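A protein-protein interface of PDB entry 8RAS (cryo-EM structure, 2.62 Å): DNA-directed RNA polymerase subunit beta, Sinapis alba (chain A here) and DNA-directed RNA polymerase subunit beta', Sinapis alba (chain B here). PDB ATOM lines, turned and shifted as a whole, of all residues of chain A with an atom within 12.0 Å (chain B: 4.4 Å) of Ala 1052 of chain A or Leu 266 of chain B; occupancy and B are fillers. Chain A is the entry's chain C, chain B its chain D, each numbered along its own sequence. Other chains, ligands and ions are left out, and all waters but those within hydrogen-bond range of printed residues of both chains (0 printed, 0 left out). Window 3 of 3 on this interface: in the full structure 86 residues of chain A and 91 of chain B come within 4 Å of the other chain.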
ATOM      1  N   LEU A1043     -26.525 -11.491   8.925  1.00  0.00           N
ATOM      2  CA  LEU A1043     -25.836 -12.598   8.274  1.00  0.00           C
ATOM      3  C   LEU A1043     -24.472 -12.166   7.751  1.00  0.00           C
ATOM      4  O   LEU A1043     -23.495 -12.917   7.849  1.00  0.00           O
ATOM      5  CB  LEU A1043     -26.712 -13.149   7.149  1.00  0.00           C
ATOM      6  CG  LEU A1043     -26.102 -13.928   5.987  1.00  0.00           C
ATOM      7  CD1 LEU A1043     -25.583 -15.267   6.451  1.00  0.00           C
ATOM      8  CD2 LEU A1043     -27.142 -14.111   4.899  1.00  0.00           C
ATOM      9  N   LEU A1044     -24.383 -10.955   7.198  1.00  0.00           N
ATOM     10  CA  LEU A1044     -23.107 -10.459   6.694  1.00  0.00           C
ATOM     11  C   LEU A1044     -22.128 -10.179   7.828  1.00  0.00           C
ATOM     12  O   LEU A1044     -20.918 -10.382   7.674  1.00  0.00           O
ATOM     13  CB  LEU A1044     -23.329  -9.200   5.857  1.00  0.00           C
ATOM     14  CG  LEU A1044     -22.078  -8.486   5.344  1.00  0.00           C
ATOM     15  CD1 LEU A1044     -21.654  -9.047   3.999  1.00  0.00           C
ATOM     16  CD2 LEU A1044     -22.310  -6.988   5.257  1.00  0.00           C
ATOM     17  N   VAL A1045     -22.628  -9.703   8.970  1.00  0.00           N
ATOM     18  CA  VAL A1045     -21.750  -9.392  10.096  1.00  0.00           C
ATOM     19  C   VAL A1045     -21.062 -10.654  10.602  1.00  0.00           C
ATOM     20  O   VAL A1045     -19.856 -10.654  10.871  1.00  0.00           O
ATOM     21  CB  VAL A1045     -22.542  -8.689  11.213  1.00  0.00           C
ATOM     22  CG1 VAL A1045     -21.693  -8.555  12.461  1.00  0.00           C
ATOM     23  CG2 VAL A1045     -23.006  -7.326  10.748  1.00  0.00           C
ATOM     24  N   ARG A1046     -21.816 -11.747  10.736  1.00  0.00           N
ATOM     25  CA  ARG A1046     -21.228 -13.000  11.198  1.00  0.00           C
ATOM     26  C   ARG A1046     -20.180 -13.516  10.219  1.00  0.00           C
ATOM     27  O   ARG A1046     -19.139 -14.038  10.631  1.00  0.00           O
ATOM     28  CB  ARG A1046     -22.318 -14.048  11.410  1.00  0.00           C
ATOM     29  CG  ARG A1046     -23.340 -13.688  12.471  1.00  0.00           C
ATOM     30  CD  ARG A1046     -22.677 -13.367  13.797  1.00  0.00           C
ATOM     31  NE  ARG A1046     -23.628 -12.843  14.770  1.00  0.00           N
ATOM     32  CZ  ARG A1046     -24.143 -11.622  14.733  1.00  0.00           C
ATOM     33  NH1 ARG A1046     -23.818 -10.762  13.782  1.00  0.00           N
ATOM     34  NH2 ARG A1046     -25.004 -11.253  15.675  1.00  0.00           N
ATOM     35  N   GLU A1047     -20.443 -13.387   8.916  1.00  0.00           N
ATOM     36  CA  GLU A1047     -19.470 -13.820   7.920  1.00  0.00           C
ATOM     37  C   GLU A1047     -18.193 -12.995   8.002  1.00  0.00           C
ATOM     38  O   GLU A1047     -17.087 -13.534   7.874  1.00  0.00           O
ATOM     39  CB  GLU A1047     -20.075 -13.733   6.522  1.00  0.00           C
ATOM     40  CG  GLU A1047     -21.281 -14.624   6.324  1.00  0.00           C
ATOM     41  CD  GLU A1047     -21.808 -14.577   4.909  1.00  0.00           C
ATOM     42  OE1 GLU A1047     -21.011 -14.788   3.973  1.00  0.00           O
ATOM     43  OE2 GLU A1047     -23.015 -14.327   4.732  1.00  0.00           O
ATOM     44  N   LEU A1048     -18.323 -11.681   8.202  1.00  0.00           N
ATOM     45  CA  LEU A1048     -17.142 -10.850   8.399  1.00  0.00           C
ATOM     46  C   LEU A1048     -16.434 -11.192   9.702  1.00  0.00           C
ATOM     47  O   LEU A1048     -15.208 -11.064   9.791  1.00  0.00           O
ATOM     48  CB  LEU A1048     -17.525  -9.373   8.372  1.00  0.00           C
ATOM     49  CG  LEU A1048     -18.005  -8.840   7.025  1.00  0.00           C
ATOM     50  CD1 LEU A1048     -18.461  -7.400   7.155  1.00  0.00           C
ATOM     51  CD2 LEU A1048     -16.909  -8.967   5.986  1.00  0.00           C
ATOM     52  N   ARG A1049     -17.184 -11.619  10.720  1.00  0.00           N
ATOM     53  CA  ARG A1049     -16.559 -12.095  11.947  1.00  0.00           C
ATOM     54  C   ARG A1049     -15.714 -13.332  11.690  1.00  0.00           C
ATOM     55  O   ARG A1049     -14.674 -13.518  12.330  1.00  0.00           O
ATOM     56  CB  ARG A1049     -17.621 -12.395  13.002  1.00  0.00           C
ATOM     57  CG  ARG A1049     -18.239 -11.177  13.654  1.00  0.00           C
ATOM     58  CD  ARG A1049     -19.174 -11.593  14.773  1.00  0.00           C
ATOM     59  NE  ARG A1049     -19.810 -10.449  15.414  1.00  0.00           N
ATOM     60  CZ  ARG A1049     -20.600 -10.533  16.475  1.00  0.00           C
ATOM     61  NH1 ARG A1049     -20.873 -11.695  17.044  1.00  0.00           N
ATOM     62  NH2 ARG A1049     -21.130  -9.422  16.978  1.00  0.00           N
ATOM     63  N   SER A1050     -16.141 -14.187  10.759  1.00  0.00           N
ATOM     64  CA  SER A1050     -15.389 -15.387  10.421  1.00  0.00           C
ATOM     65  C   SER A1050     -14.090 -15.081   9.691  1.00  0.00           C
ATOM     66  O   SER A1050     -13.237 -15.967   9.583  1.00  0.00           O
ATOM     67  CB  SER A1050     -16.251 -16.320   9.572  1.00  0.00           C
ATOM     68  OG  SER A1050     -17.469 -16.618  10.231  1.00  0.00           O
ATOM     69  N   LEU A1051     -13.923 -13.859   9.186  1.00  0.00           N
ATOM     70  CA  LEU A1051     -12.665 -13.403   8.616  1.00  0.00           C
ATOM     71  C   LEU A1051     -11.882 -12.534   9.591  1.00  0.00           C
ATOM     72  O   LEU A1051     -11.038 -11.738   9.164  1.00  0.00           O
ATOM     73  CB  LEU A1051     -12.915 -12.648   7.312  1.00  0.00           C
ATOM     74  CG  LEU A1051     -13.367 -13.499   6.125  1.00  0.00           C
ATOM     75  CD1 LEU A1051     -14.310 -12.716   5.233  1.00  0.00           C
ATOM     76  CD2 LEU A1051     -12.165 -13.990   5.341  1.00  0.00           C
ATOM     77  N   ALA A1052     -12.158 -12.667  10.889  1.00  0.00           N
ATOM     78  CA  ALA A1052     -11.486 -11.910  11.945  1.00  0.00           C
ATOM     79  C   ALA A1052     -11.693 -10.406  11.791  1.00  0.00           C
ATOM     80  O   ALA A1052     -10.801  -9.613  12.100  1.00  0.00           O
ATOM     81  CB  ALA A1052      -9.993 -12.243  12.005  1.00  0.00           C
ATOM     82  N   LEU A1053     -12.868 -10.002  11.316  1.00  0.00           N
ATOM     83  CA  LEU A1053     -13.216  -8.598  11.147  1.00  0.00           C
ATOM     84  C   LEU A1053     -14.475  -8.301  11.946  1.00  0.00           C
ATOM     85  O   LEU A1053     -15.450  -9.052  11.872  1.00  0.00           O
ATOM     86  CB  LEU A1053     -13.436  -8.256   9.671  1.00  0.00           C
ATOM     87  CG  LEU A1053     -12.347  -8.661   8.676  1.00  0.00           C
ATOM     88  CD1 LEU A1053     -12.655  -8.098   7.300  1.00  0.00           C
ATOM     89  CD2 LEU A1053     -10.980  -8.202   9.147  1.00  0.00           C
ATOM     90  N   GLU A1054     -14.457  -7.208  12.702  1.00  0.00           N
ATOM     91  CA  GLU A1054     -15.600  -6.795  13.505  1.00  0.00           C
ATOM     92  C   GLU A1054     -16.224  -5.545  12.903  1.00  0.00           C
ATOM     93  O   GLU A1054     -15.522  -4.571  12.611  1.00  0.00           O
ATOM     94  CB  GLU A1054     -15.191  -6.548  14.960  1.00  0.00           C
ATOM     95  CG  GLU A1054     -14.003  -5.622  15.137  1.00  0.00           C
ATOM     96  CD  GLU A1054     -14.014  -4.923  16.480  1.00  0.00           C
ATOM     97  OE1 GLU A1054     -14.980  -5.125  17.245  1.00  0.00           O
ATOM     98  OE2 GLU A1054     -13.060  -4.172  16.768  1.00  0.00           O
ATOM     99  N   LEU A1055     -17.540  -5.580  12.715  1.00  0.00           N
ATOM    100  CA  LEU A1055     -18.303  -4.481  12.134  1.00  0.00           C
ATOM    101  C   LEU A1055     -19.398  -4.092  13.118  1.00  0.00           C
ATOM    102  O   LEU A1055     -20.341  -4.858  13.338  1.00  0.00           O
ATOM    103  CB  LEU A1055     -18.887  -4.880  10.780  1.00  0.00           C
ATOM    104  CG  LEU A1055     -19.880  -3.925  10.116  1.00  0.00           C
ATOM    105  CD1 LEU A1055     -19.178  -2.739   9.486  1.00  0.00           C
ATOM    106  CD2 LEU A1055     -20.697  -4.669   9.075  1.00  0.00           C
ATOM    107  N   ASN A1056     -19.273  -2.907  13.707  1.00  0.00           N
ATOM    108  CA  ASN A1056     -20.204  -2.425  14.716  1.00  0.00           C
ATOM    109  C   ASN A1056     -20.945  -1.202  14.199  1.00  0.00           C
ATOM    110  O   ASN A1056     -20.361  -0.357  13.519  1.00  0.00           O
ATOM    111  CB  ASN A1056     -19.472  -2.070  16.012  1.00  0.00           C
ATOM    112  CG  ASN A1056     -18.625  -3.207  16.533  1.00  0.00           C
ATOM    113  OD1 ASN A1056     -19.091  -4.034  17.315  1.00  0.00           O
ATOM    114  ND2 ASN A1056     -17.370  -3.254  16.101  1.00  0.00           N
ATOM    115  N   GLY B  13     -12.951  -3.223  11.643  1.00  0.00           N
ATOM    116  CA  GLY B  13     -11.675  -3.227  12.326  1.00  0.00           C
ATOM    117  C   GLY B  13     -11.128  -4.626  12.500  1.00  0.00           C
ATOM    118  O   GLY B  13     -11.898  -5.582  12.625  1.00  0.00           O
ATOM    119  N   LEU B  14      -9.806  -4.769  12.500  1.00  0.00           N
ATOM    120  CA  LEU B  14      -9.208  -6.061  12.802  1.00  0.00           C
ATOM    121  C   LEU B  14      -9.497  -6.444  14.247  1.00  0.00           C
ATOM    122  O   LEU B  14      -9.417  -5.615  15.156  1.00  0.00           O
ATOM    123  CB  LEU B  14      -7.701  -6.027  12.552  1.00  0.00           C
ATOM    124  CG  LEU B  14      -7.208  -6.797  11.328  1.00  0.00           C
ATOM    125  CD1 LEU B  14      -5.697  -6.719  11.233  1.00  0.00           C
ATOM    126  CD2 LEU B  14      -7.663  -8.243  11.392  1.00  0.00           C
ATOM    127  N   VAL B  15      -9.830  -7.710  14.454  1.00  0.00           N
ATOM    128  CA  VAL B  15     -10.283  -8.184  15.751  1.00  0.00           C
ATOM    129  C   VAL B  15      -9.101  -8.754  16.526  1.00  0.00           C
ATOM    130  O   VAL B  15      -8.089  -9.169  15.957  1.00  0.00           O
ATOM    131  CB  VAL B  15     -11.404  -9.232  15.592  1.00  0.00           C
ATOM    132  CG1 VAL B  15     -10.824 -10.573  15.186  1.00  0.00           C
ATOM    133  CG2 VAL B  15     -12.210  -9.354  16.858  1.00  0.00           C
ATOM    134  N   LEU B 109      -6.214 -22.655  18.160  1.00  0.00           N
ATOM    135  CA  LEU B 109      -5.096 -23.179  17.391  1.00  0.00           C
ATOM    136  C   LEU B 109      -3.871 -23.330  18.282  1.00  0.00           C
ATOM    137  O   LEU B 109      -3.529 -22.421  19.044  1.00  0.00           O
ATOM    138  CB  LEU B 109      -4.783 -22.257  16.213  1.00  0.00           C
ATOM    139  CG  LEU B 109      -5.958 -21.900  15.304  1.00  0.00           C
ATOM    140  CD1 LEU B 109      -5.716 -20.567  14.623  1.00  0.00           C
ATOM    141  CD2 LEU B 109      -6.190 -22.991  14.276  1.00  0.00           C
ATOM    142  N   PRO B 112       0.069 -20.218  16.133  1.00  0.00           N
ATOM    143  CA  PRO B 112      -0.531 -19.093  15.410  1.00  0.00           C
ATOM    144  C   PRO B 112      -0.414 -19.285  13.905  1.00  0.00           C
ATOM    145  O   PRO B 112       0.585 -19.802  13.402  1.00  0.00           O
ATOM    146  CB  PRO B 112       0.282 -17.887  15.892  1.00  0.00           C
ATOM    147  CG  PRO B 112       1.575 -18.463  16.361  1.00  0.00           C
ATOM    148  CD  PRO B 112       1.235 -19.806  16.931  1.00  0.00           C
ATOM    149  N   VAL B 113      -1.449 -18.860  13.188  1.00  0.00           N
ATOM    150  CA  VAL B 113      -1.480 -18.917  11.732  1.00  0.00           C
ATOM    151  C   VAL B 113      -1.747 -17.517  11.201  1.00  0.00           C
ATOM    152  O   VAL B 113      -2.599 -16.792  11.725  1.00  0.00           O
ATOM    153  CB  VAL B 113      -2.531 -19.923  11.210  1.00  0.00           C
ATOM    154  CG1 VAL B 113      -2.200 -21.327  11.686  1.00  0.00           C
ATOM    155  CG2 VAL B 113      -3.929 -19.533  11.651  1.00  0.00           C
ATOM    156  N   THR B 114      -0.993 -17.128  10.179  1.00  0.00           N
ATOM    157  CA  THR B 114      -1.152 -15.801   9.604  1.00  0.00           C
ATOM    158  C   THR B 114      -2.461 -15.704   8.830  1.00  0.00           C
ATOM    159  O   THR B 114      -2.996 -16.699   8.335  1.00  0.00           O
ATOM    160  CB  THR B 114       0.025 -15.470   8.686  1.00  0.00           C
ATOM    161  OG1 THR B 114      -0.089 -14.118   8.227  1.00  0.00           O
ATOM    162  CG2 THR B 114       0.051 -16.403   7.488  1.00  0.00           C
ATOM    163  N   HIS B 115      -2.988 -14.486   8.745  1.00  0.00           N
ATOM    164  CA  HIS B 115      -4.170 -14.231   7.938  1.00  0.00           C
ATOM    165  C   HIS B 115      -3.754 -14.084   6.481  1.00  0.00           C
ATOM    166  O   HIS B 115      -2.863 -13.293   6.159  1.00  0.00           O
ATOM    167  CB  HIS B 115      -4.891 -12.974   8.426  1.00  0.00           C
ATOM    168  CG  HIS B 115      -6.313 -12.873   7.972  1.00  0.00           C
ATOM    169  ND1 HIS B 115      -6.669 -12.825   6.641  1.00  0.00           N
ATOM    170  CD2 HIS B 115      -7.469 -12.805   8.672  1.00  0.00           C
ATOM    171  CE1 HIS B 115      -7.984 -12.735   6.543  1.00  0.00           C
ATOM    172  NE2 HIS B 115      -8.493 -12.720   7.761  1.00  0.00           N
ATOM    173  N   TRP B 263      -2.375  -8.730  15.351  1.00  0.00           N
ATOM    174  CA  TRP B 263      -3.651  -9.374  15.070  1.00  0.00           C
ATOM    175  C   TRP B 263      -3.729  -9.890  13.643  1.00  0.00           C
ATOM    176  O   TRP B 263      -4.644 -10.656  13.324  1.00  0.00           O
ATOM    177  CB  TRP B 263      -4.804  -8.405  15.329  1.00  0.00           C
ATOM    178  CG  TRP B 263      -4.885  -7.926  16.742  1.00  0.00           C
ATOM    179  CD1 TRP B 263      -4.245  -8.450  17.823  1.00  0.00           C
ATOM    180  CD2 TRP B 263      -5.654  -6.821  17.225  1.00  0.00           C
ATOM    181  NE1 TRP B 263      -4.567  -7.740  18.953  1.00  0.00           N
ATOM    182  CE2 TRP B 263      -5.432  -6.734  18.612  1.00  0.00           C
ATOM    183  CE3 TRP B 263      -6.509  -5.897  16.621  1.00  0.00           C
ATOM    184  CZ2 TRP B 263      -6.033  -5.760  19.403  1.00  0.00           C
ATOM    185  CZ3 TRP B 263      -7.106  -4.934  17.408  1.00  0.00           C
ATOM    186  CH2 TRP B 263      -6.865  -4.872  18.784  1.00  0.00           C
ATOM    187  N   MET B 264      -2.794  -9.484  12.785  1.00  0.00           N
ATOM    188  CA  MET B 264      -2.698  -9.978  11.421  1.00  0.00           C
ATOM    189  C   MET B 264      -2.316 -11.451  11.367  1.00  0.00           C
ATOM    190  O   MET B 264      -2.414 -12.062  10.299  1.00  0.00           O
ATOM    191  CB  MET B 264      -1.676  -9.136  10.665  1.00  0.00           C
ATOM    192  CG  MET B 264      -2.150  -7.719  10.410  1.00  0.00           C
ATOM    193  SD  MET B 264      -0.808  -6.594  10.001  1.00  0.00           S
ATOM    194  CE  MET B 264      -0.827  -6.704   8.226  1.00  0.00           C
ATOM    195  N   VAL B 265      -1.875 -12.021  12.485  1.00  0.00           N
ATOM    196  CA  VAL B 265      -1.620 -13.448  12.620  1.00  0.00           C
ATOM    197  C   VAL B 265      -2.575 -13.986  13.674  1.00  0.00           C
ATOM    198  O   VAL B 265      -2.638 -13.456  14.788  1.00  0.00           O
ATOM    199  CB  VAL B 265      -0.156 -13.730  12.999  1.00  0.00           C
ATOM    200  CG1 VAL B 265       0.000 -15.150  13.500  1.00  0.00           C
ATOM    201  CG2 VAL B 265       0.743 -13.485  11.806  1.00  0.00           C
ATOM    202  N   LEU B 266      -3.315 -15.032  13.322  1.00  0.00           N
ATOM    203  CA  LEU B 266      -4.443 -15.482  14.124  1.00  0.00           C
ATOM    204  C   LEU B 266      -3.996 -16.467  15.195  1.00  0.00           C
ATOM    205  O   LEU B 266      -3.281 -17.432  14.905  1.00  0.00           O
ATOM    206  CB  LEU B 266      -5.506 -16.123  13.234  1.00  0.00           C
ATOM    207  CG  LEU B 266      -6.114 -15.216  12.165  1.00  0.00           C
ATOM    208  CD1 LEU B 266      -7.003 -16.016  11.232  1.00  0.00           C
ATOM    209  CD2 LEU B 266      -6.888 -14.085  12.810  1.00  0.00           C
ATOM    210  N   CYS B 267      -4.422 -16.218  16.431  1.00  0.00           N
ATOM    211  CA  CYS B 267      -4.257 -17.166  17.525  1.00  0.00           C
ATOM    212  C   CYS B 267      -5.511 -17.986  17.782  1.00  0.00           C
ATOM    213  O   CYS B 267      -5.412 -19.122  18.253  1.00  0.00           O
ATOM    214  CB  CYS B 267      -3.864 -16.433  18.812  1.00  0.00           C
ATOM    215  SG  CYS B 267      -2.194 -15.750  18.801  1.00  0.00           S
ATOM    216  N   LEU B 268      -6.684 -17.433  17.482  1.00  0.00           N
ATOM    217  CA  LEU B 268      -7.948 -18.142  17.581  1.00  0.00           C
ATOM    218  C   LEU B 268      -8.699 -17.989  16.268  1.00  0.00           C
ATOM    219  O   LEU B 268      -8.500 -17.028  15.522  1.00  0.00           O
ATOM    220  CB  LEU B 268      -8.805 -17.622  18.741  1.00  0.00           C
ATOM    221  CG  LEU B 268      -8.154 -17.595  20.123  1.00  0.00           C
ATOM    222  CD1 LEU B 268      -9.104 -16.998  21.137  1.00  0.00           C
ATOM    223  CD2 LEU B 268      -7.728 -18.988  20.546  1.00  0.00           C
ATOM    224  N   LEU B 269      -9.562 -18.955  15.985  1.00  0.00           N
ATOM    225  CA  LEU B 269     -10.333 -18.965  14.743  1.00  0.00           C
ATOM    226  C   LEU B 269     -11.820 -18.935  15.052  1.00  0.00           C
ATOM    227  O   LEU B 269     -12.380 -19.966  15.472  1.00  0.00           O
ATOM    228  CB  LEU B 269      -9.988 -20.194  13.904  1.00  0.00           C
ATOM    229  CG  LEU B 269     -10.342 -20.110  12.422  1.00  0.00           C
ATOM    230  CD1 LEU B 269      -9.284 -19.331  11.666  1.00  0.00           C
ATOM    231  CD2 LEU B 269     -10.499 -21.500  11.840  1.00  0.00           C
ATOM    232  N   LEU B 336     -10.334 -19.438   4.680  1.00  0.00           N
ATOM    233  CA  LEU B 336     -10.467 -17.986   4.606  1.00  0.00           C
ATOM    234  C   LEU B 336     -10.537 -17.498   3.165  1.00  0.00           C
ATOM    235  O   LEU B 336     -11.437 -16.730   2.809  1.00  0.00           O
ATOM    236  CB  LEU B 336      -9.306 -17.316   5.341  1.00  0.00           C
ATOM    237  CG  LEU B 336      -9.390 -17.274   6.868  1.00  0.00           C
ATOM    238  CD1 LEU B 336      -8.489 -16.184   7.417  1.00  0.00           C
ATOM    239  CD2 LEU B 336     -10.822 -17.069   7.330  1.00  0.00           C
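NE2 of His 115 of chain B is in hydrogen-bond range of O of Leu 1051 of chain A (3.1 Å). The backbone NH of Val 15 of chain B is in hydrogen-bond range of the backbone carbonyl oxygen of Ala 1052 of chain A. The backbone NH (N) of Glu 1054 of chain A is in hydrogen-bond range of the backbone carbonyl oxygen (O) of Gly 13 of chain B, 3.0 Å away.
O of Arg 1046 of chain A is in hydrogen-bond range of OG of Ser 1050 of chain A, 3.1 Å away. N of Leu 1053 of chain A sits at hydrogen-bond distance from O of Leu 1048 of chain A (3.0 Å). The side-chain amide nitrogen (ND2) of Asn 1056 of chain A sits at hydrogen-bond distance from the side-chain carboxylate (OE1) of Glu 1054 of chain A, 3.2 Å away. O of Val 113 of chain B sits at hydrogen-bond distance from N of Leu 266 of chain B, 2.5 Å away. N of His 115 of chain B is in hydrogen-bond range of O of Met 264 of chain B (2.9 Å).
Of the 16 printed residues of chain B, 6 touch a printed residue of chain A. Printed residues of chain B that touch a printed residue of chain A: Gly 13, Leu 14, Val 15, His 115, Leu 266 and Leu 336. Printed residues of chain A that touch a printed residue of chain B: Ser 1050, Leu 1051, Ala 1052, Leu 1053 and Glu 1054. Hydrophobic or aromatic side chains of chain A within 4 Å of the printed part of chain B: Leu 1051 and Ala 1052. Among the printed residues, 8 pairs touch across the chains. Among the printed residues, no Asp or Glu carboxylate lies within 4 Å of a Lys or Arg side-chain nitrogen of the other chain.
Among the printed residues, pairs that only touch across the chains: Ser 1050 of chain A with Leu 336 of chain B, Ala 1052 of chain A with Leu 14 of chain B, Leu 1053 of chain A with Gly 13 of chain B, Ala 1052 of chain A with Leu 266 of chain B and Leu 1051 of chain A with Leu 336 of chain B.
Ala 1052 of chain A touches just these residues of chain B: Leu 14 (3.5 Å), Val 15 (3.2 Å) and Leu 266 (3.7 Å). Printed residues of chain B within 4 Å of Leu 1053 of chain A: Gly 13. Printed residues of chain B within 4 Å of Glu 1054 of chain A: Gly 13 (3.0 Å). Of chain A, only Ala 1052 comes within 4 Å of Val 15 of chain B. No residue of chain A comes within 4 Å of Leu 109 of chain B. No residue of chain A comes within 4 Å of Pro 112 of chain B. No residue of chain A comes within 4 Å of Val 113 of chain B. Thr 114 of chain B touches none of the printed residues of chain A. Printed residues of chain A within 4 Å of His 115 of chain B: Leu 1051. No residue of chain A comes within 4 Å of Val 265 of chain B. Of chain A, only Ala 1052 comes within 4 Å of Leu 266 of chain B. No residue of chain A comes within 4 Å of Cys 267 of chain B. No residue of chain A comes within 4 Å of Leu 268 of chain B. Printed residues of chain A within 4 Å of Leu 336 of chain B: Ser 1050 and Leu 1051. The nearest printed residue of chain B that does not touch Ala 1052 of chain A is Gly 13 of chain B (4.2 Å). The nearest residue of chain A that does not touch Leu 266 of chain B is Leu 1051 of chain A (6.0 Å). The nearest printed residue of chain B that does not touch Glu 1054 of chain A is Leu 14 of chain B (4.2 Å).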
